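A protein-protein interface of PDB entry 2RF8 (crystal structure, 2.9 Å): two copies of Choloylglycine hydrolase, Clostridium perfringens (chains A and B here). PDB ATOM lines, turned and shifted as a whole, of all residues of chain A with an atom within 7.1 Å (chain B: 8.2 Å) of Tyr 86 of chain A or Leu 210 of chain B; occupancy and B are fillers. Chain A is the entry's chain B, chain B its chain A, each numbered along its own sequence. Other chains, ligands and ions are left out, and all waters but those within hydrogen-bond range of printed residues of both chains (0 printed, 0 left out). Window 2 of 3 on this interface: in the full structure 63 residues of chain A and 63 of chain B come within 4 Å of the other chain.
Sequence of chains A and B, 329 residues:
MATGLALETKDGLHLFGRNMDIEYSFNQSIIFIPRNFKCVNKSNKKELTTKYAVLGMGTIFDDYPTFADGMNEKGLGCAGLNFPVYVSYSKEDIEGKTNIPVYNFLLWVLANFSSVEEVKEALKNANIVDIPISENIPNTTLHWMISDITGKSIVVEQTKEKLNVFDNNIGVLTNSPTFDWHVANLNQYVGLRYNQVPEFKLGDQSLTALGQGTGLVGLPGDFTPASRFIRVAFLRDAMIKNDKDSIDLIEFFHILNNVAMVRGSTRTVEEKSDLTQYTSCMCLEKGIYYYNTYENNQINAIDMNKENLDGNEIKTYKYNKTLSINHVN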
ATOM      1  N   ASN A  82     -22.634  28.231  -0.285  1.00  0.00           N
ATOM      2  CA  ASN A  82     -22.876  29.351  -1.195  1.00  0.00           C
ATOM      3  C   ASN A  82     -24.182  29.216  -1.972  1.00  0.00           C
ATOM      4  O   ASN A  82     -24.586  28.113  -2.340  1.00  0.00           O
ATOM      5  CB  ASN A  82     -21.704  29.520  -2.164  1.00  0.00           C
ATOM      6  CG  ASN A  82     -21.676  30.889  -2.814  1.00  0.00           C
ATOM      7  OD1 ASN A  82     -21.682  31.917  -2.133  1.00  0.00           O
ATOM      8  ND2 ASN A  82     -21.636  30.911  -4.141  1.00  0.00           N
ATOM      9  N   PHE A  83     -24.828  30.352  -2.222  1.00  0.00           N
ATOM     10  CA  PHE A  83     -26.145  30.385  -2.852  1.00  0.00           C
ATOM     11  C   PHE A  83     -26.283  31.637  -3.730  1.00  0.00           C
ATOM     12  O   PHE A  83     -27.037  32.543  -3.386  1.00  0.00           O
ATOM     13  CB  PHE A  83     -27.217  30.357  -1.756  1.00  0.00           C
ATOM     14  CG  PHE A  83     -28.562  29.858  -2.213  1.00  0.00           C
ATOM     15  CD1 PHE A  83     -28.671  28.759  -3.062  1.00  0.00           C
ATOM     16  CD2 PHE A  83     -29.726  30.467  -1.757  1.00  0.00           C
ATOM     17  CE1 PHE A  83     -29.920  28.296  -3.472  1.00  0.00           C
ATOM     18  CE2 PHE A  83     -30.978  30.011  -2.158  1.00  0.00           C
ATOM     19  CZ  PHE A  83     -31.075  28.921  -3.018  1.00  0.00           C
ATOM     20  N   PRO A  84     -25.560  31.678  -4.874  1.00  0.00           N
ATOM     21  CA  PRO A  84     -25.393  32.862  -5.735  1.00  0.00           C
ATOM     22  C   PRO A  84     -26.643  33.730  -5.937  1.00  0.00           C
ATOM     23  O   PRO A  84     -26.676  34.870  -5.464  1.00  0.00           O
ATOM     24  CB  PRO A  84     -24.934  32.258  -7.062  1.00  0.00           C
ATOM     25  CG  PRO A  84     -24.153  31.084  -6.656  1.00  0.00           C
ATOM     26  CD  PRO A  84     -24.834  30.519  -5.432  1.00  0.00           C
ATOM     27  N   VAL A  85     -27.643  33.205  -6.644  1.00  0.00           N
ATOM     28  CA  VAL A  85     -28.914  33.913  -6.823  1.00  0.00           C
ATOM     29  C   VAL A  85     -30.011  33.140  -6.079  1.00  0.00           C
ATOM     30  O   VAL A  85     -29.705  32.308  -5.219  1.00  0.00           O
ATOM     31  CB  VAL A  85     -29.279  34.116  -8.325  1.00  0.00           C
ATOM     32  CG1 VAL A  85     -30.099  35.392  -8.505  1.00  0.00           C
ATOM     33  CG2 VAL A  85     -28.025  34.176  -9.201  1.00  0.00           C
ATOM     34  N   TYR A  86     -31.275  33.423  -6.398  1.00  0.00           N
ATOM     35  CA  TYR A  86     -32.439  32.762  -5.778  1.00  0.00           C
ATOM     36  C   TYR A  86     -32.563  33.037  -4.272  1.00  0.00           C
ATOM     37  O   TYR A  86     -33.448  32.493  -3.603  1.00  0.00           O
ATOM     38  CB  TYR A  86     -32.444  31.247  -6.059  1.00  0.00           C
ATOM     39  CG  TYR A  86     -32.385  30.885  -7.528  1.00  0.00           C
ATOM     40  CD1 TYR A  86     -33.536  30.902  -8.321  1.00  0.00           C
ATOM     41  CD2 TYR A  86     -31.178  30.523  -8.127  1.00  0.00           C
ATOM     42  CE1 TYR A  86     -33.485  30.571  -9.673  1.00  0.00           C
ATOM     43  CE2 TYR A  86     -31.114  30.191  -9.480  1.00  0.00           C
ATOM     44  CZ  TYR A  86     -32.270  30.217 -10.246  1.00  0.00           C
ATOM     45  OH  TYR A  86     -32.210  29.890 -11.584  1.00  0.00           O
ATOM     46  N   VAL A  87     -31.678  33.890  -3.757  1.00  0.00           N
ATOM     47  CA  VAL A  87     -31.699  34.306  -2.354  1.00  0.00           C
ATOM     48  C   VAL A  87     -31.917  35.815  -2.242  1.00  0.00           C
ATOM     49  O   VAL A  87     -31.271  36.605  -2.937  1.00  0.00           O
ATOM     50  CB  VAL A  87     -30.405  33.861  -1.590  1.00  0.00           C
ATOM     51  CG1 VAL A  87     -29.158  34.458  -2.230  1.00  0.00           C
ATOM     52  CG2 VAL A  87     -30.471  34.236  -0.111  1.00  0.00           C
ATOM     53  N   SER A  88     -32.846  36.204  -1.375  1.00  0.00           N
ATOM     54  CA  SER A  88     -33.092  37.610  -1.098  1.00  0.00           C
ATOM     55  C   SER A  88     -33.096  37.859   0.404  1.00  0.00           C
ATOM     56  O   SER A  88     -33.980  37.383   1.124  1.00  0.00           O
ATOM     57  CB  SER A  88     -34.410  38.070  -1.726  1.00  0.00           C
ATOM     58  OG  SER A  88     -34.630  39.451  -1.494  1.00  0.00           O
ATOM     59  N   GLU A 157     -33.406  27.872   3.138  1.00  0.00           N
ATOM     60  CA  GLU A 157     -33.165  28.836   2.068  1.00  0.00           C
ATOM     61  C   GLU A 157     -34.170  29.978   2.150  1.00  0.00           C
ATOM     62  O   GLU A 157     -35.379  29.746   2.229  1.00  0.00           O
ATOM     63  CB  GLU A 157     -33.259  28.163   0.693  1.00  0.00           C
ATOM     64  CG  GLU A 157     -32.200  27.095   0.425  1.00  0.00           C
ATOM     65  CD  GLU A 157     -32.398  26.374  -0.900  1.00  0.00           C
ATOM     66  OE1 GLU A 157     -33.485  26.493  -1.505  1.00  0.00           O
ATOM     67  OE2 GLU A 157     -31.457  25.677  -1.337  1.00  0.00           O
ATOM     68  N   GLN A 158     -33.665  31.209   2.140  1.00  0.00           N
ATOM     69  CA  GLN A 158     -34.529  32.382   2.127  1.00  0.00           C
ATOM     70  C   GLN A 158     -34.678  32.907   0.710  1.00  0.00           C
ATOM     71  O   GLN A 158     -33.707  33.352   0.096  1.00  0.00           O
ATOM     72  CB  GLN A 158     -34.009  33.485   3.061  1.00  0.00           C
ATOM     73  CG  GLN A 158     -34.906  34.730   3.110  1.00  0.00           C
ATOM     74  CD  GLN A 158     -34.834  35.479   4.432  1.00  0.00           C
ATOM     75  OE1 GLN A 158     -34.891  34.879   5.509  1.00  0.00           O
ATOM     76  NE2 GLN A 158     -34.728  36.802   4.354  1.00  0.00           N
ATOM     77  N   THR A 159     -35.901  32.837   0.197  1.00  0.00           N
ATOM     78  CA  THR A 159     -36.231  33.426  -1.091  1.00  0.00           C
ATOM     79  C   THR A 159     -36.971  34.738  -0.867  1.00  0.00           C
ATOM     80  O   THR A 159     -37.340  35.069   0.264  1.00  0.00           O
ATOM     81  CB  THR A 159     -37.095  32.482  -1.953  1.00  0.00           C
ATOM     82  OG1 THR A 159     -38.299  32.158  -1.246  1.00  0.00           O
ATOM     83  CG2 THR A 159     -36.335  31.199  -2.284  1.00  0.00           C
ATOM     84  N   LYS A 160     -37.182  35.474  -1.955  1.00  0.00           N
ATOM     85  CA  LYS A 160     -37.865  36.771  -1.946  1.00  0.00           C
ATOM     86  C   LYS A 160     -39.206  36.731  -1.205  1.00  0.00           C
ATOM     87  O   LYS A 160     -39.540  37.661  -0.466  1.00  0.00           O
ATOM     88  CB  LYS A 160     -38.066  37.276  -3.383  1.00  0.00           C
ATOM     89  CG  LYS A 160     -36.936  36.900  -4.353  1.00  0.00           C
ATOM     90  CD  LYS A 160     -37.211  35.566  -5.062  1.00  0.00           C
ATOM     91  CE  LYS A 160     -35.984  34.652  -5.064  1.00  0.00           C
ATOM     92  NZ  LYS A 160     -34.810  35.225  -5.781  1.00  0.00           N
ATOM     93  N   ASN A 175     -25.322  23.828  -4.219  1.00  0.00           N
ATOM     94  CA  ASN A 175     -25.585  25.255  -4.392  1.00  0.00           C
ATOM     95  C   ASN A 175     -26.724  25.485  -5.379  1.00  0.00           C
ATOM     96  O   ASN A 175     -27.478  24.556  -5.696  1.00  0.00           O
ATOM     97  CB  ASN A 175     -24.350  25.967  -4.945  1.00  0.00           C
ATOM     98  CG  ASN A 175     -23.077  25.588  -4.217  1.00  0.00           C
ATOM     99  OD1 ASN A 175     -22.214  24.907  -4.775  1.00  0.00           O
ATOM    100  ND2 ASN A 175     -22.956  26.019  -2.963  1.00  0.00           N
ATOM    101  N   SER A 176     -26.829  26.726  -5.865  1.00  0.00           N
ATOM    102  CA  SER A 176     -27.874  27.145  -6.802  1.00  0.00           C
ATOM    103  C   SER A 176     -28.029  26.169  -7.975  1.00  0.00           C
ATOM    104  O   SER A 176     -27.030  25.649  -8.480  1.00  0.00           O
ATOM    105  CB  SER A 176     -27.582  28.558  -7.317  1.00  0.00           C
ATOM    106  OG  SER A 176     -27.666  29.503  -6.264  1.00  0.00           O
ATOM    107  N   PRO A 177     -29.278  25.918  -8.422  1.00  0.00           N
ATOM    108  CA  PRO A 177     -30.560  26.503  -8.003  1.00  0.00           C
ATOM    109  C   PRO A 177     -31.070  26.031  -6.636  1.00  0.00           C
ATOM    110  O   PRO A 177     -30.337  25.383  -5.884  1.00  0.00           O
ATOM    111  CB  PRO A 177     -31.532  26.049  -9.106  1.00  0.00           C
ATOM    112  CG  PRO A 177     -30.682  25.448 -10.184  1.00  0.00           C
ATOM    113  CD  PRO A 177     -29.474  24.936  -9.500  1.00  0.00           C
ATOM    114  N   THR A 178     -32.323  26.369  -6.334  1.00  0.00           N
ATOM    115  CA  THR A 178     -32.955  26.037  -5.056  1.00  0.00           C
ATOM    116  C   THR A 178     -33.040  24.529  -4.824  1.00  0.00           C
ATOM    117  O   THR A 178     -32.974  23.743  -5.768  1.00  0.00           O
ATOM    118  CB  THR A 178     -34.373  26.641  -4.952  1.00  0.00           C
ATOM    119  OG1 THR A 178     -35.192  26.129  -6.010  1.00  0.00           O
ATOM    120  CG2 THR A 178     -34.328  28.164  -5.036  1.00  0.00           C
ATOM    121  N   TRP A 181     -35.537  22.411  -6.846  1.00  0.00           N
ATOM    122  CA  TRP A 181     -35.066  22.206  -8.215  1.00  0.00           C
ATOM    123  C   TRP A 181     -34.196  20.952  -8.310  1.00  0.00           C
ATOM    124  O   TRP A 181     -34.389  20.124  -9.203  1.00  0.00           O
ATOM    125  CB  TRP A 181     -34.279  23.429  -8.701  1.00  0.00           C
ATOM    126  CG  TRP A 181     -33.870  23.365 -10.149  1.00  0.00           C
ATOM    127  CD1 TRP A 181     -34.514  23.943 -11.204  1.00  0.00           C
ATOM    128  CD2 TRP A 181     -32.727  22.691 -10.699  1.00  0.00           C
ATOM    129  NE1 TRP A 181     -33.849  23.668 -12.375  1.00  0.00           N
ATOM    130  CE2 TRP A 181     -32.748  22.905 -12.095  1.00  0.00           C
ATOM    131  CE3 TRP A 181     -31.685  21.931 -10.147  1.00  0.00           C
ATOM    132  CZ2 TRP A 181     -31.771  22.383 -12.950  1.00  0.00           C
ATOM    133  CZ3 TRP A 181     -30.714  21.410 -10.998  1.00  0.00           C
ATOM    134  CH2 TRP A 181     -30.766  21.640 -12.385  1.00  0.00           C
ATOM    135  N   THR A 224     -20.172  21.455 -11.620  1.00  0.00           N
ATOM    136  CA  THR A 224     -21.291  22.366 -11.350  1.00  0.00           C
ATOM    137  C   THR A 224     -22.086  21.874 -10.137  1.00  0.00           C
ATOM    138  O   THR A 224     -22.101  20.670  -9.860  1.00  0.00           O
ATOM    139  CB  THR A 224     -22.242  22.507 -12.558  1.00  0.00           C
ATOM    140  OG1 THR A 224     -22.701  21.214 -12.969  1.00  0.00           O
ATOM    141  CG2 THR A 224     -21.552  23.209 -13.718  1.00  0.00           C
ATOM    142  N   PRO A 225     -22.739  22.800  -9.404  1.00  0.00           N
ATOM    143  CA  PRO A 225     -23.546  22.426  -8.241  1.00  0.00           C
ATOM    144  C   PRO A 225     -24.521  21.284  -8.531  1.00  0.00           C
ATOM    145  O   PRO A 225     -24.617  20.345  -7.736  1.00  0.00           O
ATOM    146  CB  PRO A 225     -24.305  23.714  -7.922  1.00  0.00           C
ATOM    147  CG  PRO A 225     -23.399  24.793  -8.383  1.00  0.00           C
ATOM    148  CD  PRO A 225     -22.740  24.261  -9.618  1.00  0.00           C
ATOM    149  N   GLN B 196     -14.406  29.472 -16.758  1.00  0.00           N
ATOM    150  CA  GLN B 196     -15.815  29.659 -16.442  1.00  0.00           C
ATOM    151  C   GLN B 196     -16.550  30.351 -17.584  1.00  0.00           C
ATOM    152  O   GLN B 196     -16.054  31.330 -18.147  1.00  0.00           O
ATOM    153  CB  GLN B 196     -15.964  30.462 -15.144  1.00  0.00           C
ATOM    154  CG  GLN B 196     -17.390  30.883 -14.785  1.00  0.00           C
ATOM    155  CD  GLN B 196     -18.253  29.743 -14.266  1.00  0.00           C
ATOM    156  OE1 GLN B 196     -17.845  28.578 -14.259  1.00  0.00           O
ATOM    157  NE2 GLN B 196     -19.459  30.080 -13.822  1.00  0.00           N
ATOM    158  N   VAL B 197     -17.722  29.820 -17.926  1.00  0.00           N
ATOM    159  CA  VAL B 197     -18.620  30.462 -18.880  1.00  0.00           C
ATOM    160  C   VAL B 197     -19.738  31.157 -18.090  1.00  0.00           C
ATOM    161  O   VAL B 197     -20.695  30.504 -17.658  1.00  0.00           O
ATOM    162  CB  VAL B 197     -19.195  29.456 -19.911  1.00  0.00           C
ATOM    163  CG1 VAL B 197     -19.996  30.184 -20.979  1.00  0.00           C
ATOM    164  CG2 VAL B 197     -18.075  28.654 -20.561  1.00  0.00           C
ATOM    165  N   PRO B 198     -19.612  32.488 -17.895  1.00  0.00           N
ATOM    166  CA  PRO B 198     -20.486  33.260 -17.003  1.00  0.00           C
ATOM    167  C   PRO B 198     -21.923  33.388 -17.503  1.00  0.00           C
ATOM    168  O   PRO B 198     -22.858  33.129 -16.742  1.00  0.00           O
ATOM    169  CB  PRO B 198     -19.820  34.645 -16.948  1.00  0.00           C
ATOM    170  CG  PRO B 198     -18.488  34.488 -17.595  1.00  0.00           C
ATOM    171  CD  PRO B 198     -18.604  33.347 -18.540  1.00  0.00           C
ATOM    172  N   GLU B 199     -22.098  33.791 -18.761  1.00  0.00           N
ATOM    173  CA  GLU B 199     -23.436  33.990 -19.316  1.00  0.00           C
ATOM    174  C   GLU B 199     -23.612  33.447 -20.737  1.00  0.00           C
ATOM    175  O   GLU B 199     -22.637  33.124 -21.419  1.00  0.00           O
ATOM    176  CB  GLU B 199     -23.850  35.471 -19.241  1.00  0.00           C
ATOM    177  CG  GLU B 199     -23.232  36.376 -20.305  1.00  0.00           C
ATOM    178  CD  GLU B 199     -24.182  37.477 -20.766  1.00  0.00           C
ATOM    179  OE1 GLU B 199     -24.689  38.236 -19.909  1.00  0.00           O
ATOM    180  OE2 GLU B 199     -24.419  37.587 -21.990  1.00  0.00           O
ATOM    181  N   LEU B 207     -29.203  33.708 -19.989  1.00  0.00           N
ATOM    182  CA  LEU B 207     -28.828  32.532 -19.214  1.00  0.00           C
ATOM    183  C   LEU B 207     -27.535  32.798 -18.460  1.00  0.00           C
ATOM    184  O   LEU B 207     -26.495  33.052 -19.065  1.00  0.00           O
ATOM    185  CB  LEU B 207     -28.684  31.299 -20.117  1.00  0.00           C
ATOM    186  CG  LEU B 207     -29.890  30.862 -20.959  1.00  0.00           C
ATOM    187  CD1 LEU B 207     -29.540  29.623 -21.774  1.00  0.00           C
ATOM    188  CD2 LEU B 207     -31.129  30.613 -20.101  1.00  0.00           C
ATOM    189  N   THR B 208     -27.613  32.750 -17.135  1.00  0.00           N
ATOM    190  CA  THR B 208     -26.457  33.010 -16.287  1.00  0.00           C
ATOM    191  C   THR B 208     -26.037  31.743 -15.552  1.00  0.00           C
ATOM    192  O   THR B 208     -26.882  30.996 -15.057  1.00  0.00           O
ATOM    193  CB  THR B 208     -26.739  34.138 -15.263  1.00  0.00           C
ATOM    194  OG1 THR B 208     -27.844  33.768 -14.429  1.00  0.00           O
ATOM    195  CG2 THR B 208     -27.060  35.455 -15.971  1.00  0.00           C
ATOM    196  N   ALA B 209     -24.729  31.507 -15.496  1.00  0.00           N
ATOM    197  CA  ALA B 209     -24.168  30.375 -14.767  1.00  0.00           C
ATOM    198  C   ALA B 209     -24.486  30.481 -13.281  1.00  0.00           C
ATOM    199  O   ALA B 209     -24.297  31.536 -12.670  1.00  0.00           O
ATOM    200  CB  ALA B 209     -22.669  30.304 -14.980  1.00  0.00           C
ATOM    201  N   LEU B 210     -24.967  29.381 -12.709  1.00  0.00           N
ATOM    202  CA  LEU B 210     -25.384  29.350 -11.307  1.00  0.00           C
ATOM    203  C   LEU B 210     -24.289  28.806 -10.386  1.00  0.00           C
ATOM    204  O   LEU B 210     -24.441  28.794  -9.162  1.00  0.00           O
ATOM    205  CB  LEU B 210     -26.683  28.548 -11.156  1.00  0.00           C
ATOM    206  CG  LEU B 210     -27.820  28.934 -12.115  1.00  0.00           C
ATOM    207  CD1 LEU B 210     -28.982  27.954 -12.027  1.00  0.00           C
ATOM    208  CD2 LEU B 210     -28.294  30.381 -11.902  1.00  0.00           C
ATOM    209  N   GLY B 211     -23.186  28.369 -10.988  1.00  0.00           N
ATOM    210  CA  GLY B 211     -22.035  27.868 -10.248  1.00  0.00           C
ATOM    211  C   GLY B 211     -20.788  27.799 -11.105  1.00  0.00           C
ATOM    212  O   GLY B 211     -20.807  28.174 -12.277  1.00  0.00           O
ATOM    213  N   GLN B 212     -19.698  27.319 -10.515  1.00  0.00           N
ATOM    214  CA  GLN B 212     -18.438  27.163 -11.233  1.00  0.00           C
ATOM    215  C   GLN B 212     -18.375  25.835 -11.978  1.00  0.00           C
ATOM    216  O   GLN B 212     -19.081  24.885 -11.635  1.00  0.00           O
ATOM    217  CB  GLN B 212     -17.250  27.276 -10.273  1.00  0.00           C
ATOM    218  CG  GLN B 212     -16.997  28.679  -9.725  1.00  0.00           C
ATOM    219  CD  GLN B 212     -16.536  29.672 -10.783  1.00  0.00           C
ATOM    220  OE1 GLN B 212     -16.840  30.861 -10.701  1.00  0.00           O
ATOM    221  NE2 GLN B 212     -15.795  29.188 -11.779  1.00  0.00           N
ATOM    222  N   GLY B 213     -17.526  25.785 -13.001  1.00  0.00           N
ATOM    223  CA  GLY B 213     -17.287  24.563 -13.764  1.00  0.00           C
ATOM    224  C   GLY B 213     -18.284  24.295 -14.877  1.00  0.00           C
ATOM    225  O   GLY B 213     -18.512  23.141 -15.242  1.00  0.00           O
ATOM    226  N   THR B 214     -18.869  25.360 -15.419  1.00  0.00           N
ATOM    227  CA  THR B 214     -19.851  25.249 -16.501  1.00  0.00           C
ATOM    228  C   THR B 214     -19.216  24.864 -17.835  1.00  0.00           C
ATOM    229  O   THR B 214     -19.866  24.253 -18.686  1.00  0.00           O
ATOM    230  CB  THR B 214     -20.637  26.557 -16.700  1.00  0.00           C
ATOM    231  OG1 THR B 214     -19.724  27.636 -16.941  1.00  0.00           O
ATOM    232  CG2 THR B 214     -21.483  26.869 -15.480  1.00  0.00           C
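Leu 210 of chain B touches just these residues of chain A: Pro 84, Tyr 86, Ser 176 and Pro 177.
Printed residues of chain B within 4 Å of Ser 176 of chain A: Leu 210.
Of the printed residues of chain A, Gly 211 of chain B touches Pro 225 (3.7 Å).
Ser 88 of chain A touches none of the printed residues of chain B.
Leu 207 of chain B touches none of the printed residues of chain A.
Among the printed residues, merely in contact across the chains: Pro 84 of chain A with Leu 210 of chain B (3.4 Å), Tyr 86 of chain A with Leu 210 of chain B (3.7 Å), Ser 176 of chain A with Leu 210 of chain B (3.7 Å), Pro 177 of chain A with Leu 210 of chain B (3.5 Å), Thr 224 of chain A with Gln 212 of chain B (3.4 Å), Thr 224 of chain A with Gly 213 of chain B (3.4 Å), Thr 224 of chain A with Thr 214 of chain B (3.8 Å) and Pro 225 of chain A with Gly 211 of chain B (3.7 Å).
The side-chain hydroxyl of Thr 214 of chain B sits at hydrogen-bond distance from the side-chain amide oxygen of Gln 196 of chain B (3.4 Å).
O of Gly 211 of chain B lies within hydrogen-bond range of NE2 of Gln 196 of chain B (2.8 Å).
The side-chain amide oxygen (OE1) of Gln 196 of chain B is in hydrogen-bond range of the backbone NH (N) of Gly 213 of chain B (3.1 Å).
The side-chain hydroxyl (OG1) of Thr 214 of chain B is in hydrogen-bond range of the backbone carbonyl oxygen (O) of Val 197 of chain B.
The side-chain amide oxygen of Gln 196 of chain B is in hydrogen-bond range of the side-chain amide nitrogen of Gln 212 of chain B (3.3 Å).
No position is printed for both chains.
Of the 8 pairs that touch across the chains among the printed residues, none has its exchanged pair printed and touching as well.
Hydrophobic or aromatic side chains of chain B that line the printed part of chain A: Leu 210.
Among the printed residues, 8 pairs touch across the chains.
Among the printed residues, no Asp or Glu carboxylate lies within 4 Å of a Lys or Arg side-chain nitrogen of the other chain.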
